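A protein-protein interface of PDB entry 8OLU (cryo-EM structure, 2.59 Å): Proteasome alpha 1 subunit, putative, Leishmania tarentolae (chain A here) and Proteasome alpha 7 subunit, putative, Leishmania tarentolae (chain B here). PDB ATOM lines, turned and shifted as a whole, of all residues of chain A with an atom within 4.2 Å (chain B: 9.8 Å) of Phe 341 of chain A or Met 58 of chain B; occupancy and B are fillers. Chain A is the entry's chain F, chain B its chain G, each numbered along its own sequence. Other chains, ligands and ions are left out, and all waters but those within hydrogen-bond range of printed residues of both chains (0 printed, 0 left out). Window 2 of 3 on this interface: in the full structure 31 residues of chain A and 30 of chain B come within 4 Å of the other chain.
Of chain B, only Met 58 (3.8 Å) comes within 4 Å of Leu 337 of chain A. No residue of chain B comes within 4 Å of Glu 342 of chain A. Of the printed residues of chain A, Glu 60 of chain B touches Tyr 321 (3.8 Å) and Lys 322 (3.5 Å). Printed residues of chain A within 4 Å of Leu 59 of chain B: Tyr 321 and Lys 322. Of the printed residues of chain A, Arg 57 of chain B touches Glu 338 (2.6 Å) and Phe 341 (3.3 Å). Printed residues of chain B within 4 Å of Tyr 321 of chain A: Ser 56 (3.6 Å), Met 58 (3.5 Å), Leu 59 (3.4 Å) and Glu 60 (3.8 Å). Of the printed residues of chain A, Ser 56 of chain B touches Tyr 321 (3.6 Å). Thr 55 of chain B touches none of the printed residues of chain A.
The side-chain amino group (NZ) of Lys 322 of chain A is in salt-bridge range of the side-chain carboxylate (OE1) of Glu 60 of chain B. O of Met 58 of chain B is in hydrogen-bond range of N of Lys 322 of chain A, 3.0 Å away. The backbone carbonyl oxygen (O) of Ala 323 of chain A sits close to the side-chain sulfur (SD) of Met 58 of chain B (3.7 Å). OE2 of Glu 338 of chain A is in salt-bridge range of NH1 of Arg 57 of chain B (2.6 Å).
Among the printed residues, pairs that only touch across the chains: Tyr 321 of chain A with Ser 56 of chain B (3.6 Å), Tyr 321 of chain A with Met 58 of chain B (3.5 Å), Tyr 321 of chain A with Leu 59 of chain B (3.4 Å), Tyr 321 of chain A with Glu 60 of chain B (3.8 Å), Lys 322 of chain A with Leu 59 of chain B (3.7 Å), Leu 337 of chain A with Met 58 of chain B (3.8 Å), Phe 341 of chain A with Arg 57 of chain B (3.3 Å) and Phe 341 of chain A with Met 58 of chain B (3.6 Å).
Printed residues of chain A that touch a printed residue of chain B: Tyr 321, Lys 322, Ala 323, Leu 337, Glu 338 and Phe 341. Of the 13 printed residues of chain B, 5 touch a printed residue of chain A. Printed residues of chain B that touch a printed residue of chain A: Ser 56, Arg 57, Met 58, Leu 59 and Glu 60. Hydrophobic or aromatic side chains of chain B that line the printed part of chain A: Met 58 and Leu 59. Among the printed residues, 12 pairs touch across the chains.
The side-chain hydroxyl of Ser 56 of chain B lies close to the backbone NH of Met 58 of chain B, 3.3 Å away.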
ATOM      1  N   TYR A 321      26.926 -13.250 -24.926  1.00  0.00           N
ATOM      2  CA  TYR A 321      26.772 -11.911 -24.426  1.00  0.00           C
ATOM      3  C   TYR A 321      26.916 -10.925 -25.556  1.00  0.00           C
ATOM      4  O   TYR A 321      27.370 -11.301 -26.637  1.00  0.00           O
ATOM      5  CB  TYR A 321      27.864 -11.583 -23.439  1.00  0.00           C
ATOM      6  CG  TYR A 321      27.581 -11.971 -22.018  1.00  0.00           C
ATOM      7  CD1 TYR A 321      26.743 -11.202 -21.259  1.00  0.00           C
ATOM      8  CD2 TYR A 321      28.200 -13.027 -21.406  1.00  0.00           C
ATOM      9  CE1 TYR A 321      26.504 -11.467 -19.930  1.00  0.00           C
ATOM     10  CE2 TYR A 321      27.918 -13.357 -20.088  1.00  0.00           C
ATOM     11  CZ  TYR A 321      27.051 -12.583 -19.338  1.00  0.00           C
ATOM     12  OH  TYR A 321      26.781 -12.805 -17.995  1.00  0.00           O
ATOM     13  N   LYS A 322      26.451  -9.712 -25.285  1.00  0.00           N
ATOM     14  CA  LYS A 322      26.669  -8.530 -26.088  1.00  0.00           C
ATOM     15  C   LYS A 322      27.867  -7.772 -25.517  1.00  0.00           C
ATOM     16  O   LYS A 322      28.592  -7.089 -26.225  1.00  0.00           O
ATOM     17  CB  LYS A 322      25.484  -7.566 -25.950  1.00  0.00           C
ATOM     18  CG  LYS A 322      24.158  -8.025 -26.534  1.00  0.00           C
ATOM     19  CD  LYS A 322      23.102  -6.947 -26.359  1.00  0.00           C
ATOM     20  CE  LYS A 322      21.667  -7.405 -26.548  1.00  0.00           C
ATOM     21  NZ  LYS A 322      21.549  -8.125 -27.831  1.00  0.00           N
ATOM     22  N   ALA A 323      27.980  -7.796 -24.198  1.00  0.00           N
ATOM     23  CA  ALA A 323      29.175  -7.307 -23.540  1.00  0.00           C
ATOM     24  C   ALA A 323      29.273  -7.960 -22.182  1.00  0.00           C
ATOM     25  O   ALA A 323      28.277  -8.416 -21.677  1.00  0.00           O
ATOM     26  CB  ALA A 323      29.162  -5.812 -23.414  1.00  0.00           C
ATOM     27  N   LEU A 337      29.412  -1.248 -18.530  1.00  0.00           N
ATOM     28  CA  LEU A 337      28.983  -1.781 -19.799  1.00  0.00           C
ATOM     29  C   LEU A 337      27.466  -1.707 -19.878  1.00  0.00           C
ATOM     30  O   LEU A 337      26.946  -1.514 -20.968  1.00  0.00           O
ATOM     31  CB  LEU A 337      29.479  -3.205 -19.889  1.00  0.00           C
ATOM     32  CG  LEU A 337      30.945  -3.347 -20.242  1.00  0.00           C
ATOM     33  CD1 LEU A 337      31.330  -4.815 -20.153  1.00  0.00           C
ATOM     34  CD2 LEU A 337      31.261  -2.773 -21.634  1.00  0.00           C
ATOM     35  N   GLU A 338      26.780  -1.808 -18.733  1.00  0.00           N
ATOM     36  CA  GLU A 338      25.325  -1.796 -18.708  1.00  0.00           C
ATOM     37  C   GLU A 338      24.756  -0.451 -19.156  1.00  0.00           C
ATOM     38  O   GLU A 338      23.640  -0.413 -19.653  1.00  0.00           O
ATOM     39  CB  GLU A 338      24.822  -2.175 -17.314  1.00  0.00           C
ATOM     40  CG  GLU A 338      24.989  -3.668 -17.029  1.00  0.00           C
ATOM     41  CD  GLU A 338      24.547  -4.183 -15.662  1.00  0.00           C
ATOM     42  OE1 GLU A 338      25.290  -5.014 -15.088  1.00  0.00           O
ATOM     43  OE2 GLU A 338      23.450  -3.776 -15.181  1.00  0.00           O
ATOM     44  N   ARG A 339      25.492   0.650 -18.965  1.00  0.00           N
ATOM     45  CA  ARG A 339      25.024   1.953 -19.407  1.00  0.00           C
ATOM     46  C   ARG A 339      25.085   2.007 -20.927  1.00  0.00           C
ATOM     47  O   ARG A 339      24.166   2.483 -21.586  1.00  0.00           O
ATOM     48  CB  ARG A 339      25.854   3.104 -18.823  1.00  0.00           C
ATOM     49  CG  ARG A 339      25.550   3.455 -17.369  1.00  0.00           C
ATOM     50  CD  ARG A 339      26.232   4.743 -16.889  1.00  0.00           C
ATOM     51  NE  ARG A 339      27.658   4.633 -16.526  1.00  0.00           N
ATOM     52  CZ  ARG A 339      28.141   4.235 -15.337  1.00  0.00           C
ATOM     53  NH1 ARG A 339      29.445   4.206 -15.111  1.00  0.00           N
ATOM     54  NH2 ARG A 339      27.319   3.866 -14.366  1.00  0.00           N
ATOM     55  N   HIS A 340      26.177   1.506 -21.492  1.00  0.00           N
ATOM     56  CA  HIS A 340      26.522   1.858 -22.855  1.00  0.00           C
ATOM     57  C   HIS A 340      26.219   0.741 -23.846  1.00  0.00           C
ATOM     58  O   HIS A 340      26.294   0.979 -25.052  1.00  0.00           O
ATOM     59  CB  HIS A 340      27.986   2.317 -22.906  1.00  0.00           C
ATOM     60  CG  HIS A 340      28.214   3.585 -22.142  1.00  0.00           C
ATOM     61  ND1 HIS A 340      28.966   3.671 -20.996  1.00  0.00           N
ATOM     62  CD2 HIS A 340      27.665   4.816 -22.354  1.00  0.00           C
ATOM     63  CE1 HIS A 340      28.911   4.918 -20.527  1.00  0.00           C
ATOM     64  NE2 HIS A 340      28.100   5.642 -21.353  1.00  0.00           N
ATOM     65  N   PHE A 341      25.849  -0.456 -23.374  1.00  0.00           N
ATOM     66  CA  PHE A 341      25.950  -1.627 -24.238  1.00  0.00           C
ATOM     67  C   PHE A 341      24.902  -1.602 -25.346  1.00  0.00           C
ATOM     68  O   PHE A 341      25.114  -2.225 -26.371  1.00  0.00           O
ATOM     69  CB  PHE A 341      25.828  -2.948 -23.482  1.00  0.00           C
ATOM     70  CG  PHE A 341      24.412  -3.352 -23.150  1.00  0.00           C
ATOM     71  CD1 PHE A 341      23.732  -4.278 -23.932  1.00  0.00           C
ATOM     72  CD2 PHE A 341      23.753  -2.815 -22.050  1.00  0.00           C
ATOM     73  CE1 PHE A 341      22.439  -4.671 -23.610  1.00  0.00           C
ATOM     74  CE2 PHE A 341      22.456  -3.193 -21.743  1.00  0.00           C
ATOM     75  CZ  PHE A 341      21.799  -4.120 -22.523  1.00  0.00           C
ATOM     76  N   GLU A 342      23.789  -0.889 -25.156  1.00  0.00           N
ATOM     77  CA  GLU A 342      22.718  -0.925 -26.139  1.00  0.00           C
ATOM     78  C   GLU A 342      23.149  -0.224 -27.430  1.00  0.00           C
ATOM     79  O   GLU A 342      22.514  -0.425 -28.459  1.00  0.00           O
ATOM     80  CB  GLU A 342      21.426  -0.349 -25.551  1.00  0.00           C
ATOM     81  CG  GLU A 342      20.512  -1.396 -24.906  1.00  0.00           C
ATOM     82  CD  GLU A 342      19.772  -0.951 -23.644  1.00  0.00           C
ATOM     83  OE1 GLU A 342      19.443   0.260 -23.535  1.00  0.00           O
ATOM     84  OE2 GLU A 342      19.499  -1.819 -22.770  1.00  0.00           O
ATOM     85  N   HIS A 343      24.245   0.549 -27.389  1.00  0.00           N
ATOM     86  CA  HIS A 343      24.693   1.330 -28.538  1.00  0.00           C
ATOM     87  C   HIS A 343      25.673   0.536 -29.388  1.00  0.00           C
ATOM     88  O   HIS A 343      25.784   0.783 -30.584  1.00  0.00           O
ATOM     89  CB  HIS A 343      25.301   2.672 -28.088  1.00  0.00           C
ATOM     90  CG  HIS A 343      24.306   3.520 -27.350  1.00  0.00           C
ATOM     91  ND1 HIS A 343      24.463   3.936 -26.045  1.00  0.00           N
ATOM     92  CD2 HIS A 343      23.070   3.940 -27.763  1.00  0.00           C
ATOM     93  CE1 HIS A 343      23.379   4.617 -25.674  1.00  0.00           C
ATOM     94  NE2 HIS A 343      22.501   4.629 -26.726  1.00  0.00           N
ATOM     95  N   PHE A 344      26.340  -0.437 -28.769  1.00  0.00           N
ATOM     96  CA  PHE A 344      27.450  -1.146 -29.380  1.00  0.00           C
ATOM     97  C   PHE A 344      27.125  -1.690 -30.767  1.00  0.00           C
ATOM     98  O   PHE A 344      28.027  -1.754 -31.602  1.00  0.00           O
ATOM     99  CB  PHE A 344      27.884  -2.306 -28.492  1.00  0.00           C
ATOM    100  CG  PHE A 344      28.490  -1.931 -27.165  1.00  0.00           C
ATOM    101  CD1 PHE A 344      28.809  -0.624 -26.853  1.00  0.00           C
ATOM    102  CD2 PHE A 344      28.780  -2.914 -26.238  1.00  0.00           C
ATOM    103  CE1 PHE A 344      29.373  -0.305 -25.629  1.00  0.00           C
ATOM    104  CE2 PHE A 344      29.353  -2.591 -25.016  1.00  0.00           C
ATOM    105  CZ  PHE A 344      29.637  -1.282 -24.707  1.00  0.00           C
ATOM    106  N   HIS B  54      17.885 -14.815 -16.469  1.00  0.00           N
ATOM    107  CA  HIS B  54      19.187 -14.227 -16.729  1.00  0.00           C
ATOM    108  C   HIS B  54      19.696 -13.616 -15.447  1.00  0.00           C
ATOM    109  O   HIS B  54      18.915 -13.298 -14.565  1.00  0.00           O
ATOM    110  CB  HIS B  54      19.037 -13.179 -17.809  1.00  0.00           C
ATOM    111  CG  HIS B  54      18.430 -13.731 -19.059  1.00  0.00           C
ATOM    112  ND1 HIS B  54      18.774 -14.974 -19.569  1.00  0.00           N
ATOM    113  CD2 HIS B  54      17.501 -13.167 -19.892  1.00  0.00           C
ATOM    114  CE1 HIS B  54      18.124 -15.156 -20.711  1.00  0.00           C
ATOM    115  NE2 HIS B  54      17.314 -14.042 -20.928  1.00  0.00           N
ATOM    116  N   THR B  55      21.000 -13.433 -15.356  1.00  0.00           N
ATOM    117  CA  THR B  55      21.523 -12.685 -14.233  1.00  0.00           C
ATOM    118  C   THR B  55      21.973 -11.312 -14.724  1.00  0.00           C
ATOM    119  O   THR B  55      22.025 -10.382 -13.932  1.00  0.00           O
ATOM    120  CB  THR B  55      22.567 -13.536 -13.505  1.00  0.00           C
ATOM    121  OG1 THR B  55      22.956 -12.801 -12.340  1.00  0.00           O
ATOM    122  CG2 THR B  55      23.731 -13.917 -14.405  1.00  0.00           C
ATOM    123  N   SER B  56      22.195 -11.184 -16.040  1.00  0.00           N
ATOM    124  CA  SER B  56      22.713  -9.979 -16.660  1.00  0.00           C
ATOM    125  C   SER B  56      21.709  -9.399 -17.649  1.00  0.00           C
ATOM    126  O   SER B  56      21.022 -10.137 -18.337  1.00  0.00           O
ATOM    127  CB  SER B  56      24.045 -10.294 -17.349  1.00  0.00           C
ATOM    128  OG  SER B  56      24.622  -9.149 -18.000  1.00  0.00           O
ATOM    129  N   ARG B  57      21.733  -8.072 -17.812  1.00  0.00           N
ATOM    130  CA  ARG B  57      20.843  -7.378 -18.729  1.00  0.00           C
ATOM    131  C   ARG B  57      21.392  -7.418 -20.143  1.00  0.00           C
ATOM    132  O   ARG B  57      20.777  -6.913 -21.071  1.00  0.00           O
ATOM    133  CB  ARG B  57      20.699  -5.919 -18.279  1.00  0.00           C
ATOM    134  CG  ARG B  57      19.289  -5.357 -18.453  1.00  0.00           C
ATOM    135  CD  ARG B  57      18.834  -4.419 -17.329  1.00  0.00           C
ATOM    136  NE  ARG B  57      19.270  -3.045 -17.562  1.00  0.00           N
ATOM    137  CZ  ARG B  57      20.512  -2.599 -17.389  1.00  0.00           C
ATOM    138  NH1 ARG B  57      21.307  -3.174 -16.501  1.00  0.00           N
ATOM    139  NH2 ARG B  57      20.936  -1.559 -18.087  1.00  0.00           N
ATOM    140  N   MET B  58      22.558  -8.044 -20.294  1.00  0.00           N
ATOM    141  CA  MET B  58      23.397  -7.877 -21.464  1.00  0.00           C
ATOM    142  C   MET B  58      23.592  -9.179 -22.197  1.00  0.00           C
ATOM    143  O   MET B  58      24.455  -9.273 -23.054  1.00  0.00           O
ATOM    144  CB  MET B  58      24.776  -7.401 -21.057  1.00  0.00           C
ATOM    145  CG  MET B  58      24.771  -5.961 -20.582  1.00  0.00           C
ATOM    146  SD  MET B  58      26.455  -5.345 -20.687  1.00  0.00           S
ATOM    147  CE  MET B  58      27.191  -6.197 -19.286  1.00  0.00           C
ATOM    148  N   LEU B  59      22.767 -10.167 -21.883  1.00  0.00           N
ATOM    149  CA  LEU B  59      22.794 -11.384 -22.664  1.00  0.00           C
ATOM    150  C   LEU B  59      22.162 -11.147 -24.022  1.00  0.00           C
ATOM    151  O   LEU B  59      21.383 -10.213 -24.188  1.00  0.00           O
ATOM    152  CB  LEU B  59      22.057 -12.458 -21.879  1.00  0.00           C
ATOM    153  CG  LEU B  59      22.827 -12.917 -20.650  1.00  0.00           C
ATOM    154  CD1 LEU B  59      22.014 -13.882 -19.820  1.00  0.00           C
ATOM    155  CD2 LEU B  59      24.127 -13.576 -21.057  1.00  0.00           C
ATOM    156  N   GLU B  60      22.606 -11.970 -24.960  1.00  0.00           N
ATOM    157  CA  GLU B  60      21.982 -12.127 -26.250  1.00  0.00           C
ATOM    158  C   GLU B  60      20.711 -12.947 -26.080  1.00  0.00           C
ATOM    159  O   GLU B  60      20.677 -13.864 -25.267  1.00  0.00           O
ATOM    160  CB  GLU B  60      22.946 -12.820 -27.211  1.00  0.00           C
ATOM    161  CG  GLU B  60      23.828 -11.881 -28.010  1.00  0.00           C
ATOM    162  CD  GLU B  60      23.253 -11.127 -29.218  1.00  0.00           C
ATOM    163  OE1 GLU B  60      23.839 -10.063 -29.574  1.00  0.00           O
ATOM    164  OE2 GLU B  60      22.257 -11.596 -29.837  1.00  0.00           O
ATOM    165  N   LYS B  61      19.671 -12.625 -26.855  1.00  0.00           N
ATOM    166  CA  LYS B  61      18.463 -13.441 -26.882  1.00  0.00           C
ATOM    167  C   LYS B  61      18.795 -14.708 -27.656  1.00  0.00           C
ATOM    168  O   LYS B  61      19.328 -14.617 -28.759  1.00  0.00           O
ATOM    169  CB  LYS B  61      17.285 -12.648 -27.463  1.00  0.00           C
ATOM    170  CG  LYS B  61      16.927 -11.424 -26.626  1.00  0.00           C
ATOM    171  CD  LYS B  61      15.601 -10.747 -26.953  1.00  0.00           C
ATOM    172  CE  LYS B  61      15.242  -9.663 -25.948  1.00  0.00           C
ATOM    173  NZ  LYS B  61      13.861  -9.154 -26.125  1.00  0.00           N
ATOM    174  N   GLY B  62      18.548 -15.863 -27.016  1.00  0.00           N
ATOM    175  CA  GLY B  62      19.131 -17.131 -27.435  1.00  0.00           C
ATOM    176  C   GLY B  62      20.075 -17.719 -26.393  1.00  0.00           C
ATOM    177  O   GLY B  62      20.358 -18.903 -26.406  1.00  0.00           O
ATOM    178  N   SER B  63      20.567 -16.907 -25.467  1.00  0.00           N
ATOM    179  CA  SER B  63      21.579 -17.383 -24.537  1.00  0.00           C
ATOM    180  C   SER B  63      20.985 -18.389 -23.577  1.00  0.00           C
ATOM    181  O   SER B  63      19.939 -18.135 -23.002  1.00  0.00           O
ATOM    182  CB  SER B  63      22.224 -16.270 -23.745  1.00  0.00           C
ATOM    183  OG  SER B  63      23.017 -16.817 -22.690  1.00  0.00           O
ATOM    184  N   ASN B  64      21.748 -19.448 -23.313  1.00  0.00           N
ATOM    185  CA  ASN B  64      21.384 -20.454 -22.322  1.00  0.00           C
ATOM    186  C   ASN B  64      20.036 -21.050 -22.710  1.00  0.00           C
ATOM    187  O   ASN B  64      19.157 -21.149 -21.859  1.00  0.00           O
ATOM    188  CB  ASN B  64      21.285 -19.914 -20.881  1.00  0.00           C
ATOM    189  CG  ASN B  64      22.525 -19.171 -20.423  1.00  0.00           C
ATOM    190  OD1 ASN B  64      22.433 -18.011 -20.028  1.00  0.00           O
ATOM    191  ND2 ASN B  64      23.674 -19.833 -20.461  1.00  0.00           N
ATOM    192  N   LEU B 208      15.030 -10.320 -14.591  1.00  0.00           N
ATOM    193  CA  LEU B 208      15.289 -10.481 -16.014  1.00  0.00           C
ATOM    194  C   LEU B 208      14.894 -11.887 -16.445  1.00  0.00           C
ATOM    195  O   LEU B 208      15.404 -12.868 -15.903  1.00  0.00           O
ATOM    196  CB  LEU B 208      16.794 -10.299 -16.236  1.00  0.00           C
ATOM    197  CG  LEU B 208      17.349  -8.887 -16.463  1.00  0.00           C
ATOM    198  CD1 LEU B 208      16.338  -7.768 -16.209  1.00  0.00           C
ATOM    199  CD2 LEU B 208      18.619  -8.709 -15.630  1.00  0.00           C
ATOM    200  N   GLU B 210      13.242 -14.252 -20.040  1.00  0.00           N
ATOM    201  CA  GLU B 210      12.404 -14.529 -21.182  1.00  0.00           C
ATOM    202  C   GLU B 210      11.811 -15.902 -20.992  1.00  0.00           C
ATOM    203  O   GLU B 210      12.265 -16.674 -20.162  1.00  0.00           O
ATOM    204  CB  GLU B 210      13.139 -14.388 -22.519  1.00  0.00           C
ATOM    205  CG  GLU B 210      14.326 -15.324 -22.741  1.00  0.00           C
ATOM    206  CD  GLU B 210      15.231 -14.900 -23.902  1.00  0.00           C
ATOM    207  OE1 GLU B 210      16.418 -14.566 -23.640  1.00  0.00           O
ATOM    208  OE2 GLU B 210      14.758 -14.894 -25.074  1.00  0.00           O
